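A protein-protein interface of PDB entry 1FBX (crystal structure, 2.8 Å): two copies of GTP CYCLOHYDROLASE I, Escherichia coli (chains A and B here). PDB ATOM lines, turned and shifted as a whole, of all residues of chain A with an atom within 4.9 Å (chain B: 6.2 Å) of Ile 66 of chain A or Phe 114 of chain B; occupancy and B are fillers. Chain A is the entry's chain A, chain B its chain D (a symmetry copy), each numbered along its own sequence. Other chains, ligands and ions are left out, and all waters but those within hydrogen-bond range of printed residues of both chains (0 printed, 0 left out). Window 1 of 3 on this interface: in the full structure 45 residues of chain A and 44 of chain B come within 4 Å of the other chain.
The guanidinium group of Arg 65 of chain A sits at hydrogen-bond distance from the side-chain hydroxyl of Thr 62 of chain A (2.9 Å). The backbone NH (N) of Leu 52 of chain A is in hydrogen-bond range of the backbone carbonyl oxygen (O) of Met 47 of chain A (3.2 Å). N of Phe 75 of chain B lies close to O of Tyr 70 of chain B (3.2 Å). The backbone carbonyl oxygen (O) of Val 115 of chain B lies within hydrogen-bond range of the backbone NH (N) of Cys 110 of chain B (2.9 Å).
The guanidinium group (NE) of Arg 65 of chain A lies within hydrogen-bond range of the backbone carbonyl oxygen (O) of His 112 of chain B, at 3.1 Å. The backbone carbonyl oxygen (O) of Glu 111 of chain B sits at hydrogen-bond distance from the side-chain hydroxyl (OG1) of Thr 62 of chain A (2.7 Å).
Printed residues of chain B within 4 Å of Leu 50 of chain A: Phe 75 (3.9 Å). Pro 63 of chain A touches none of the printed residues of chain B. Printed residues of chain B within 4 Å of Arg 65 of chain A: His 112. Of the printed residues of chain B, Ile 66 of chain A touches His 113 (3.98 Å) and Phe 114 (3.8 Å). Of the printed residues of chain A, Glu 111 of chain B touches Thr 62 (2.7 Å). Printed residues of chain A within 4 Å of His 112 of chain B: Thr 62 and Arg 65. Of the printed residues of chain A, His 113 of chain B touches Ile 66 (3.98 Å) and Met 69 (3.0 Å). Phe 114 of chain B touches just these residues of chain A: Met 47 and Ile 66. The nearest printed residue of chain B that does not touch Ile 66 of chain A is His 112 of chain B (4.6 Å). The nearest residue of chain A that does not touch Phe 114 of chain B is Thr 62 of chain A (4.1 Å). The nearest printed residue of chain B that does not touch Leu 52 of chain A is Phe 114 of chain B (4.4 Å).
Position printed for both chains: 70. Of the 10 pairs that touch across the chains among the printed residues, none has its exchanged pair printed and touching as well.
Among the printed residues, pairs that only touch across the chains: Met 47 of chain A with Phe 114 of chain B (3.9 Å), Leu 50 of chain A with Phe 75 of chain B (3.9 Å), Leu 52 of chain A with Pro 148 of chain B (3.8 Å), Thr 62 of chain A with His 112 of chain B (3.6 Å), Ile 66 of chain A with His 113 of chain B (3.98 Å), Ile 66 of chain A with Phe 114 of chain B (3.8 Å), Met 69 of chain A with His 113 of chain B (3.0 Å) and Met 69 of chain A with Val 115 of chain B (3.7 Å).
Of the 12 printed residues of chain B, 7 touch a printed residue of chain A. Hydrophobic or aromatic side chains of chain A that line the printed part of chain B: Met 47, Leu 50, Leu 52, Ile 66 and Met 69. Among the printed residues, 10 pairs touch across the chains. Among the printed residues, no Asp or Glu carboxylate lies within 4 Å of a Lys or Arg side-chain nitrogen of the other chain.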
ATOM      1  N   MET A  43      -1.977  -8.928 -17.149  1.00  0.00           N
ATOM      2  CA  MET A  43      -3.146  -8.673 -17.981  1.00  0.00           C
ATOM      3  C   MET A  43      -3.184  -7.242 -18.444  1.00  0.00           C
ATOM      4  O   MET A  43      -3.722  -6.945 -19.497  1.00  0.00           O
ATOM      5  CB  MET A  43      -4.444  -8.979 -17.253  1.00  0.00           C
ATOM      6  CG  MET A  43      -4.888 -10.438 -17.347  1.00  0.00           C
ATOM      7  SD  MET A  43      -5.058 -11.060 -19.028  1.00  0.00           S
ATOM      8  CE  MET A  43      -6.096  -9.808 -19.726  1.00  0.00           C
ATOM      9  N   MET A  47      -3.547  -6.047 -22.217  1.00  0.00           N
ATOM     10  CA  MET A  47      -4.501  -5.098 -22.738  1.00  0.00           C
ATOM     11  C   MET A  47      -3.781  -3.899 -23.405  1.00  0.00           C
ATOM     12  O   MET A  47      -4.308  -3.322 -24.353  1.00  0.00           O
ATOM     13  CB  MET A  47      -5.467  -4.622 -21.642  1.00  0.00           C
ATOM     14  CG  MET A  47      -6.403  -5.687 -21.135  1.00  0.00           C
ATOM     15  SD  MET A  47      -7.445  -5.065 -19.800  1.00  0.00           S
ATOM     16  CE  MET A  47      -8.822  -4.468 -20.660  1.00  0.00           C
ATOM     17  N   LEU A  50      -2.884  -4.746 -26.893  1.00  0.00           N
ATOM     18  CA  LEU A  50      -4.017  -4.786 -27.812  1.00  0.00           C
ATOM     19  C   LEU A  50      -4.440  -3.358 -28.129  1.00  0.00           C
ATOM     20  O   LEU A  50      -5.396  -3.130 -28.836  1.00  0.00           O
ATOM     21  CB  LEU A  50      -5.185  -5.579 -27.214  1.00  0.00           C
ATOM     22  CG  LEU A  50      -4.915  -7.089 -27.108  1.00  0.00           C
ATOM     23  CD1 LEU A  50      -5.798  -7.738 -26.038  1.00  0.00           C
ATOM     24  CD2 LEU A  50      -5.130  -7.723 -28.455  1.00  0.00           C
ATOM     25  N   LEU A  52      -5.712  -1.058 -26.138  1.00  0.00           N
ATOM     26  CA  LEU A  52      -6.948  -0.588 -25.505  1.00  0.00           C
ATOM     27  C   LEU A  52      -6.598   0.526 -24.546  1.00  0.00           C
ATOM     28  O   LEU A  52      -5.593   0.450 -23.847  1.00  0.00           O
ATOM     29  CB  LEU A  52      -7.636  -1.727 -24.739  1.00  0.00           C
ATOM     30  CG  LEU A  52      -8.075  -2.901 -25.606  1.00  0.00           C
ATOM     31  CD1 LEU A  52      -8.000  -4.205 -24.856  1.00  0.00           C
ATOM     32  CD2 LEU A  52      -9.453  -2.604 -26.098  1.00  0.00           C
ATOM     33  N   THR A  62     -10.795  -3.837 -15.399  1.00  0.00           N
ATOM     34  CA  THR A  62     -10.729  -5.157 -16.010  1.00  0.00           C
ATOM     35  C   THR A  62      -9.580  -6.083 -15.631  1.00  0.00           C
ATOM     36  O   THR A  62      -9.803  -7.266 -15.345  1.00  0.00           O
ATOM     37  CB  THR A  62     -10.789  -5.069 -17.542  1.00  0.00           C
ATOM     38  OG1 THR A  62     -12.100  -4.643 -17.927  1.00  0.00           O
ATOM     39  CG2 THR A  62     -10.479  -6.434 -18.180  1.00  0.00           C
ATOM     40  N   PRO A  63      -8.342  -5.576 -15.625  1.00  0.00           N
ATOM     41  CA  PRO A  63      -7.243  -6.468 -15.273  1.00  0.00           C
ATOM     42  C   PRO A  63      -7.393  -7.012 -13.860  1.00  0.00           C
ATOM     43  O   PRO A  63      -6.971  -8.127 -13.552  1.00  0.00           O
ATOM     44  CB  PRO A  63      -6.031  -5.569 -15.433  1.00  0.00           C
ATOM     45  CG  PRO A  63      -6.470  -4.563 -16.458  1.00  0.00           C
ATOM     46  CD  PRO A  63      -7.838  -4.246 -15.996  1.00  0.00           C
ATOM     47  N   HIS A  64      -8.014  -6.221 -12.996  1.00  0.00           N
ATOM     48  CA  HIS A  64      -8.183  -6.641 -11.627  1.00  0.00           C
ATOM     49  C   HIS A  64      -9.361  -7.598 -11.498  1.00  0.00           C
ATOM     50  O   HIS A  64      -9.348  -8.488 -10.639  1.00  0.00           O
ATOM     51  CB  HIS A  64      -8.334  -5.416 -10.716  1.00  0.00           C
ATOM     52  CG  HIS A  64      -8.454  -5.761  -9.264  1.00  0.00           C
ATOM     53  ND1 HIS A  64      -7.686  -6.743  -8.669  1.00  0.00           N
ATOM     54  CD2 HIS A  64      -9.293  -5.298  -8.303  1.00  0.00           C
ATOM     55  CE1 HIS A  64      -8.054  -6.878  -7.403  1.00  0.00           C
ATOM     56  NE2 HIS A  64      -9.026  -6.015  -7.156  1.00  0.00           N
ATOM     57  N   ARG A  65     -10.378  -7.428 -12.344  1.00  0.00           N
ATOM     58  CA  ARG A  65     -11.512  -8.340 -12.317  1.00  0.00           C
ATOM     59  C   ARG A  65     -11.046  -9.681 -12.876  1.00  0.00           C
ATOM     60  O   ARG A  65     -11.348 -10.713 -12.316  1.00  0.00           O
ATOM     61  CB  ARG A  65     -12.673  -7.799 -13.142  1.00  0.00           C
ATOM     62  CG  ARG A  65     -13.410  -6.649 -12.486  1.00  0.00           C
ATOM     63  CD  ARG A  65     -14.595  -6.108 -13.280  1.00  0.00           C
ATOM     64  NE  ARG A  65     -14.172  -5.479 -14.518  1.00  0.00           N
ATOM     65  CZ  ARG A  65     -14.541  -4.258 -14.905  1.00  0.00           C
ATOM     66  NH1 ARG A  65     -15.357  -3.541 -14.135  1.00  0.00           N
ATOM     67  NH2 ARG A  65     -14.073  -3.743 -16.049  1.00  0.00           N
ATOM     68  N   ILE A  66     -10.295  -9.675 -13.971  1.00  0.00           N
ATOM     69  CA  ILE A  66      -9.813 -10.919 -14.545  1.00  0.00           C
ATOM     70  C   ILE A  66      -8.970 -11.708 -13.548  1.00  0.00           C
ATOM     71  O   ILE A  66      -9.117 -12.923 -13.401  1.00  0.00           O
ATOM     72  CB  ILE A  66      -8.969 -10.645 -15.802  1.00  0.00           C
ATOM     73  CG1 ILE A  66      -9.878 -10.088 -16.903  1.00  0.00           C
ATOM     74  CG2 ILE A  66      -8.239 -11.911 -16.245  1.00  0.00           C
ATOM     75  CD1 ILE A  66      -9.171  -9.736 -18.210  1.00  0.00           C
ATOM     76  N   ALA A  67      -8.075 -11.004 -12.864  1.00  0.00           N
ATOM     77  CA  ALA A  67      -7.174 -11.597 -11.875  1.00  0.00           C
ATOM     78  C   ALA A  67      -7.946 -12.297 -10.758  1.00  0.00           C
ATOM     79  O   ALA A  67      -7.648 -13.439 -10.386  1.00  0.00           O
ATOM     80  CB  ALA A  67      -6.290 -10.508 -11.289  1.00  0.00           C
ATOM     81  N   LYS A  68      -8.930 -11.580 -10.224  1.00  0.00           N
ATOM     82  CA  LYS A  68      -9.793 -12.070  -9.159  1.00  0.00           C
ATOM     83  C   LYS A  68     -10.630 -13.267  -9.675  1.00  0.00           C
ATOM     84  O   LYS A  68     -10.739 -14.305  -9.023  1.00  0.00           O
ATOM     85  CB  LYS A  68     -10.679 -10.908  -8.697  1.00  0.00           C
ATOM     86  CG  LYS A  68     -11.560 -11.203  -7.510  1.00  0.00           C
ATOM     87  CD  LYS A  68     -12.442 -10.001  -7.176  1.00  0.00           C
ATOM     88  CE  LYS A  68     -13.586 -10.402  -6.214  1.00  0.00           C
ATOM     89  NZ  LYS A  68     -14.493 -11.471  -6.791  1.00  0.00           N
ATOM     90  N   MET A  69     -11.192 -13.131 -10.867  1.00  0.00           N
ATOM     91  CA  MET A  69     -11.971 -14.203 -11.468  1.00  0.00           C
ATOM     92  C   MET A  69     -11.136 -15.475 -11.621  1.00  0.00           C
ATOM     93  O   MET A  69     -11.566 -16.565 -11.255  1.00  0.00           O
ATOM     94  CB  MET A  69     -12.481 -13.762 -12.842  1.00  0.00           C
ATOM     95  CG  MET A  69     -13.328 -14.787 -13.561  1.00  0.00           C
ATOM     96  SD  MET A  69     -13.370 -14.467 -15.327  1.00  0.00           S
ATOM     97  CE  MET A  69     -14.796 -13.653 -15.387  1.00  0.00           C
ATOM     98  N   TYR A  70      -9.937 -15.326 -12.167  1.00  0.00           N
ATOM     99  CA  TYR A  70      -9.059 -16.471 -12.388  1.00  0.00           C
ATOM    100  C   TYR A  70      -8.724 -17.239 -11.122  1.00  0.00           C
ATOM    101  O   TYR A  70      -8.968 -18.445 -11.041  1.00  0.00           O
ATOM    102  CB  TYR A  70      -7.762 -16.013 -13.059  1.00  0.00           C
ATOM    103  CG  TYR A  70      -7.787 -15.938 -14.577  1.00  0.00           C
ATOM    104  CD1 TYR A  70      -8.984 -15.865 -15.287  1.00  0.00           C
ATOM    105  CD2 TYR A  70      -6.599 -15.885 -15.298  1.00  0.00           C
ATOM    106  CE1 TYR A  70      -8.990 -15.735 -16.669  1.00  0.00           C
ATOM    107  CE2 TYR A  70      -6.591 -15.754 -16.677  1.00  0.00           C
ATOM    108  CZ  TYR A  70      -7.783 -15.674 -17.362  1.00  0.00           C
ATOM    109  OH  TYR A  70      -7.766 -15.503 -18.732  1.00  0.00           O
ATOM    110  N   TYR B  70      -6.198 -14.082 -29.522  1.00  0.00           N
ATOM    111  CA  TYR B  70      -6.454 -12.672 -29.196  1.00  0.00           C
ATOM    112  C   TYR B  70      -6.211 -11.719 -30.388  1.00  0.00           C
ATOM    113  O   TYR B  70      -7.080 -10.930 -30.758  1.00  0.00           O
ATOM    114  CB  TYR B  70      -5.588 -12.225 -28.003  1.00  0.00           C
ATOM    115  CG  TYR B  70      -6.074 -12.662 -26.621  1.00  0.00           C
ATOM    116  CD1 TYR B  70      -7.265 -13.378 -26.457  1.00  0.00           C
ATOM    117  CD2 TYR B  70      -5.350 -12.339 -25.475  1.00  0.00           C
ATOM    118  CE1 TYR B  70      -7.721 -13.754 -25.190  1.00  0.00           C
ATOM    119  CE2 TYR B  70      -5.788 -12.707 -24.216  1.00  0.00           C
ATOM    120  CZ  TYR B  70      -6.974 -13.412 -24.071  1.00  0.00           C
ATOM    121  OH  TYR B  70      -7.427 -13.760 -22.809  1.00  0.00           O
ATOM    122  N   ILE B  74     -10.500 -13.532 -31.991  1.00  0.00           N
ATOM    123  CA  ILE B  74     -11.524 -12.849 -31.234  1.00  0.00           C
ATOM    124  C   ILE B  74     -11.394 -11.352 -31.075  1.00  0.00           C
ATOM    125  O   ILE B  74     -12.353 -10.714 -30.683  1.00  0.00           O
ATOM    126  CB  ILE B  74     -11.823 -13.537 -29.829  1.00  0.00           C
ATOM    127  CG1 ILE B  74     -10.831 -13.101 -28.753  1.00  0.00           C
ATOM    128  CG2 ILE B  74     -11.784 -15.081 -29.940  1.00  0.00           C
ATOM    129  CD1 ILE B  74     -11.250 -13.602 -27.379  1.00  0.00           C
ATOM    130  N   PHE B  75     -10.246 -10.763 -31.390  1.00  0.00           N
ATOM    131  CA  PHE B  75     -10.127  -9.303 -31.286  1.00  0.00           C
ATOM    132  C   PHE B  75      -9.706  -8.665 -32.611  1.00  0.00           C
ATOM    133  O   PHE B  75      -9.388  -7.477 -32.667  1.00  0.00           O
ATOM    134  CB  PHE B  75      -9.123  -8.882 -30.208  1.00  0.00           C
ATOM    135  CG  PHE B  75      -9.495  -9.292 -28.827  1.00  0.00           C
ATOM    136  CD1 PHE B  75     -10.790  -9.123 -28.363  1.00  0.00           C
ATOM    137  CD2 PHE B  75      -8.533  -9.821 -27.967  1.00  0.00           C
ATOM    138  CE1 PHE B  75     -11.130  -9.479 -27.042  1.00  0.00           C
ATOM    139  CE2 PHE B  75      -8.866 -10.176 -26.651  1.00  0.00           C
ATOM    140  CZ  PHE B  75     -10.164 -10.006 -26.185  1.00  0.00           C
ATOM    141  N   THR B 109     -17.138 -10.865 -26.638  1.00  0.00           N
ATOM    142  CA  THR B 109     -16.458 -10.980 -25.321  1.00  0.00           C
ATOM    143  C   THR B 109     -16.794  -9.777 -24.438  1.00  0.00           C
ATOM    144  O   THR B 109     -16.817  -8.658 -24.930  1.00  0.00           O
ATOM    145  CB  THR B 109     -14.923 -10.942 -25.495  1.00  0.00           C
ATOM    146  OG1 THR B 109     -14.499 -11.979 -26.394  1.00  0.00           O
ATOM    147  CG2 THR B 109     -14.231 -11.089 -24.150  1.00  0.00           C
ATOM    148  N   CYS B 110     -17.043  -9.969 -23.144  1.00  0.00           N
ATOM    149  CA  CYS B 110     -17.343  -8.799 -22.303  1.00  0.00           C
ATOM    150  C   CYS B 110     -16.043  -8.094 -21.957  1.00  0.00           C
ATOM    151  O   CYS B 110     -15.064  -8.733 -21.564  1.00  0.00           O
ATOM    152  CB  CYS B 110     -18.101  -9.189 -21.020  1.00  0.00           C
ATOM    153  SG  CYS B 110     -17.238 -10.036 -19.655  1.00  0.00           S
ATOM    154  N   GLU B 111     -15.999  -6.784 -22.121  1.00  0.00           N
ATOM    155  CA  GLU B 111     -14.765  -6.104 -21.817  1.00  0.00           C
ATOM    156  C   GLU B 111     -14.423  -6.196 -20.344  1.00  0.00           C
ATOM    157  O   GLU B 111     -13.269  -5.987 -19.963  1.00  0.00           O
ATOM    158  CB  GLU B 111     -14.810  -4.645 -22.268  1.00  0.00           C
ATOM    159  CG  GLU B 111     -15.799  -3.725 -21.587  1.00  0.00           C
ATOM    160  CD  GLU B 111     -15.925  -2.378 -22.328  1.00  0.00           C
ATOM    161  OE1 GLU B 111     -15.855  -2.388 -23.588  1.00  0.00           O
ATOM    162  OE2 GLU B 111     -16.108  -1.318 -21.671  1.00  0.00           O
ATOM    163  N   HIS B 112     -15.398  -6.559 -19.517  1.00  0.00           N
ATOM    164  CA  HIS B 112     -15.158  -6.628 -18.090  1.00  0.00           C
ATOM    165  C   HIS B 112     -14.443  -7.864 -17.565  1.00  0.00           C
ATOM    166  O   HIS B 112     -13.897  -7.803 -16.490  1.00  0.00           O
ATOM    167  CB  HIS B 112     -16.465  -6.423 -17.355  1.00  0.00           C
ATOM    168  CG  HIS B 112     -17.153  -5.149 -17.722  1.00  0.00           C
ATOM    169  ND1 HIS B 112     -18.529  -5.074 -17.819  1.00  0.00           N
ATOM    170  CD2 HIS B 112     -16.615  -3.935 -17.992  1.00  0.00           C
ATOM    171  CE1 HIS B 112     -18.799  -3.822 -18.143  1.00  0.00           C
ATOM    172  NE2 HIS B 112     -17.679  -3.089 -18.261  1.00  0.00           N
ATOM    173  N   HIS B 113     -14.469  -8.994 -18.274  1.00  0.00           N
ATOM    174  CA  HIS B 113     -13.752 -10.191 -17.818  1.00  0.00           C
ATOM    175  C   HIS B 113     -13.296 -11.011 -18.979  1.00  0.00           C
ATOM    176  O   HIS B 113     -12.879 -12.145 -18.814  1.00  0.00           O
ATOM    177  CB  HIS B 113     -14.577 -11.084 -16.929  1.00  0.00           C
ATOM    178  CG  HIS B 113     -15.683 -10.371 -16.265  1.00  0.00           C
ATOM    179  ND1 HIS B 113     -15.762 -10.114 -14.913  1.00  0.00           N
ATOM    180  CD2 HIS B 113     -16.744  -9.748 -16.831  1.00  0.00           C
ATOM    181  CE1 HIS B 113     -16.843  -9.345 -14.730  1.00  0.00           C
ATOM    182  NE2 HIS B 113     -17.459  -9.104 -15.886  1.00  0.00           N
ATOM    183  N   PHE B 114     -13.389 -10.456 -20.174  1.00  0.00           N
ATOM    184  CA  PHE B 114     -12.899 -11.191 -21.315  1.00  0.00           C
ATOM    185  C   PHE B 114     -13.496 -12.589 -21.396  1.00  0.00           C
ATOM    186  O   PHE B 114     -12.822 -13.557 -21.727  1.00  0.00           O
ATOM    187  CB  PHE B 114     -11.373 -11.255 -21.222  1.00  0.00           C
ATOM    188  CG  PHE B 114     -10.695 -10.026 -21.716  1.00  0.00           C
ATOM    189  CD1 PHE B 114     -11.318  -8.791 -21.616  1.00  0.00           C
ATOM    190  CD2 PHE B 114      -9.452 -10.108 -22.321  1.00  0.00           C
ATOM    191  CE1 PHE B 114     -10.715  -7.648 -22.121  1.00  0.00           C
ATOM    192  CE2 PHE B 114      -8.834  -8.971 -22.827  1.00  0.00           C
ATOM    193  CZ  PHE B 114      -9.465  -7.737 -22.732  1.00  0.00           C
ATOM    194  N   VAL B 115     -14.776 -12.687 -21.077  1.00  0.00           N
ATOM    195  CA  VAL B 115     -15.471 -13.950 -21.167  1.00  0.00           C
ATOM    196  C   VAL B 115     -16.482 -13.879 -22.330  1.00  0.00           C
ATOM    197  O   VAL B 115     -16.874 -12.795 -22.795  1.00  0.00           O
ATOM    198  CB  VAL B 115     -16.136 -14.271 -19.839  1.00  0.00           C
ATOM    199  CG1 VAL B 115     -17.233 -15.291 -20.006  1.00  0.00           C
ATOM    200  CG2 VAL B 115     -15.096 -14.792 -18.908  1.00  0.00           C
ATOM    201  N   THR B 116     -16.862 -15.055 -22.811  1.00  0.00           N
ATOM    202  CA  THR B 116     -17.774 -15.202 -23.934  1.00  0.00           C
ATOM    203  C   THR B 116     -19.158 -14.578 -23.824  1.00  0.00           C
ATOM    204  O   THR B 116     -19.774 -14.549 -22.755  1.00  0.00           O
ATOM    205  CB  THR B 116     -17.982 -16.700 -24.260  1.00  0.00           C
ATOM    206  OG1 THR B 116     -16.725 -17.319 -24.568  1.00  0.00           O
ATOM    207  CG2 THR B 116     -18.924 -16.852 -25.426  1.00  0.00           C
ATOM    208  N   PRO B 148     -13.292  -6.367 -27.458  1.00  0.00           N
ATOM    209  CA  PRO B 148     -13.746  -6.479 -26.068  1.00  0.00           C
ATOM    210  C   PRO B 148     -14.963  -5.578 -26.131  1.00  0.00           C
ATOM    211  O   PRO B 148     -14.856  -4.478 -26.653  1.00  0.00           O
ATOM    212  CB  PRO B 148     -12.622  -5.822 -25.282  1.00  0.00           C
ATOM    213  CG  PRO B 148     -11.408  -5.911 -26.224  1.00  0.00           C
ATOM    214  CD  PRO B 148     -12.033  -5.611 -27.550  1.00  0.00           C
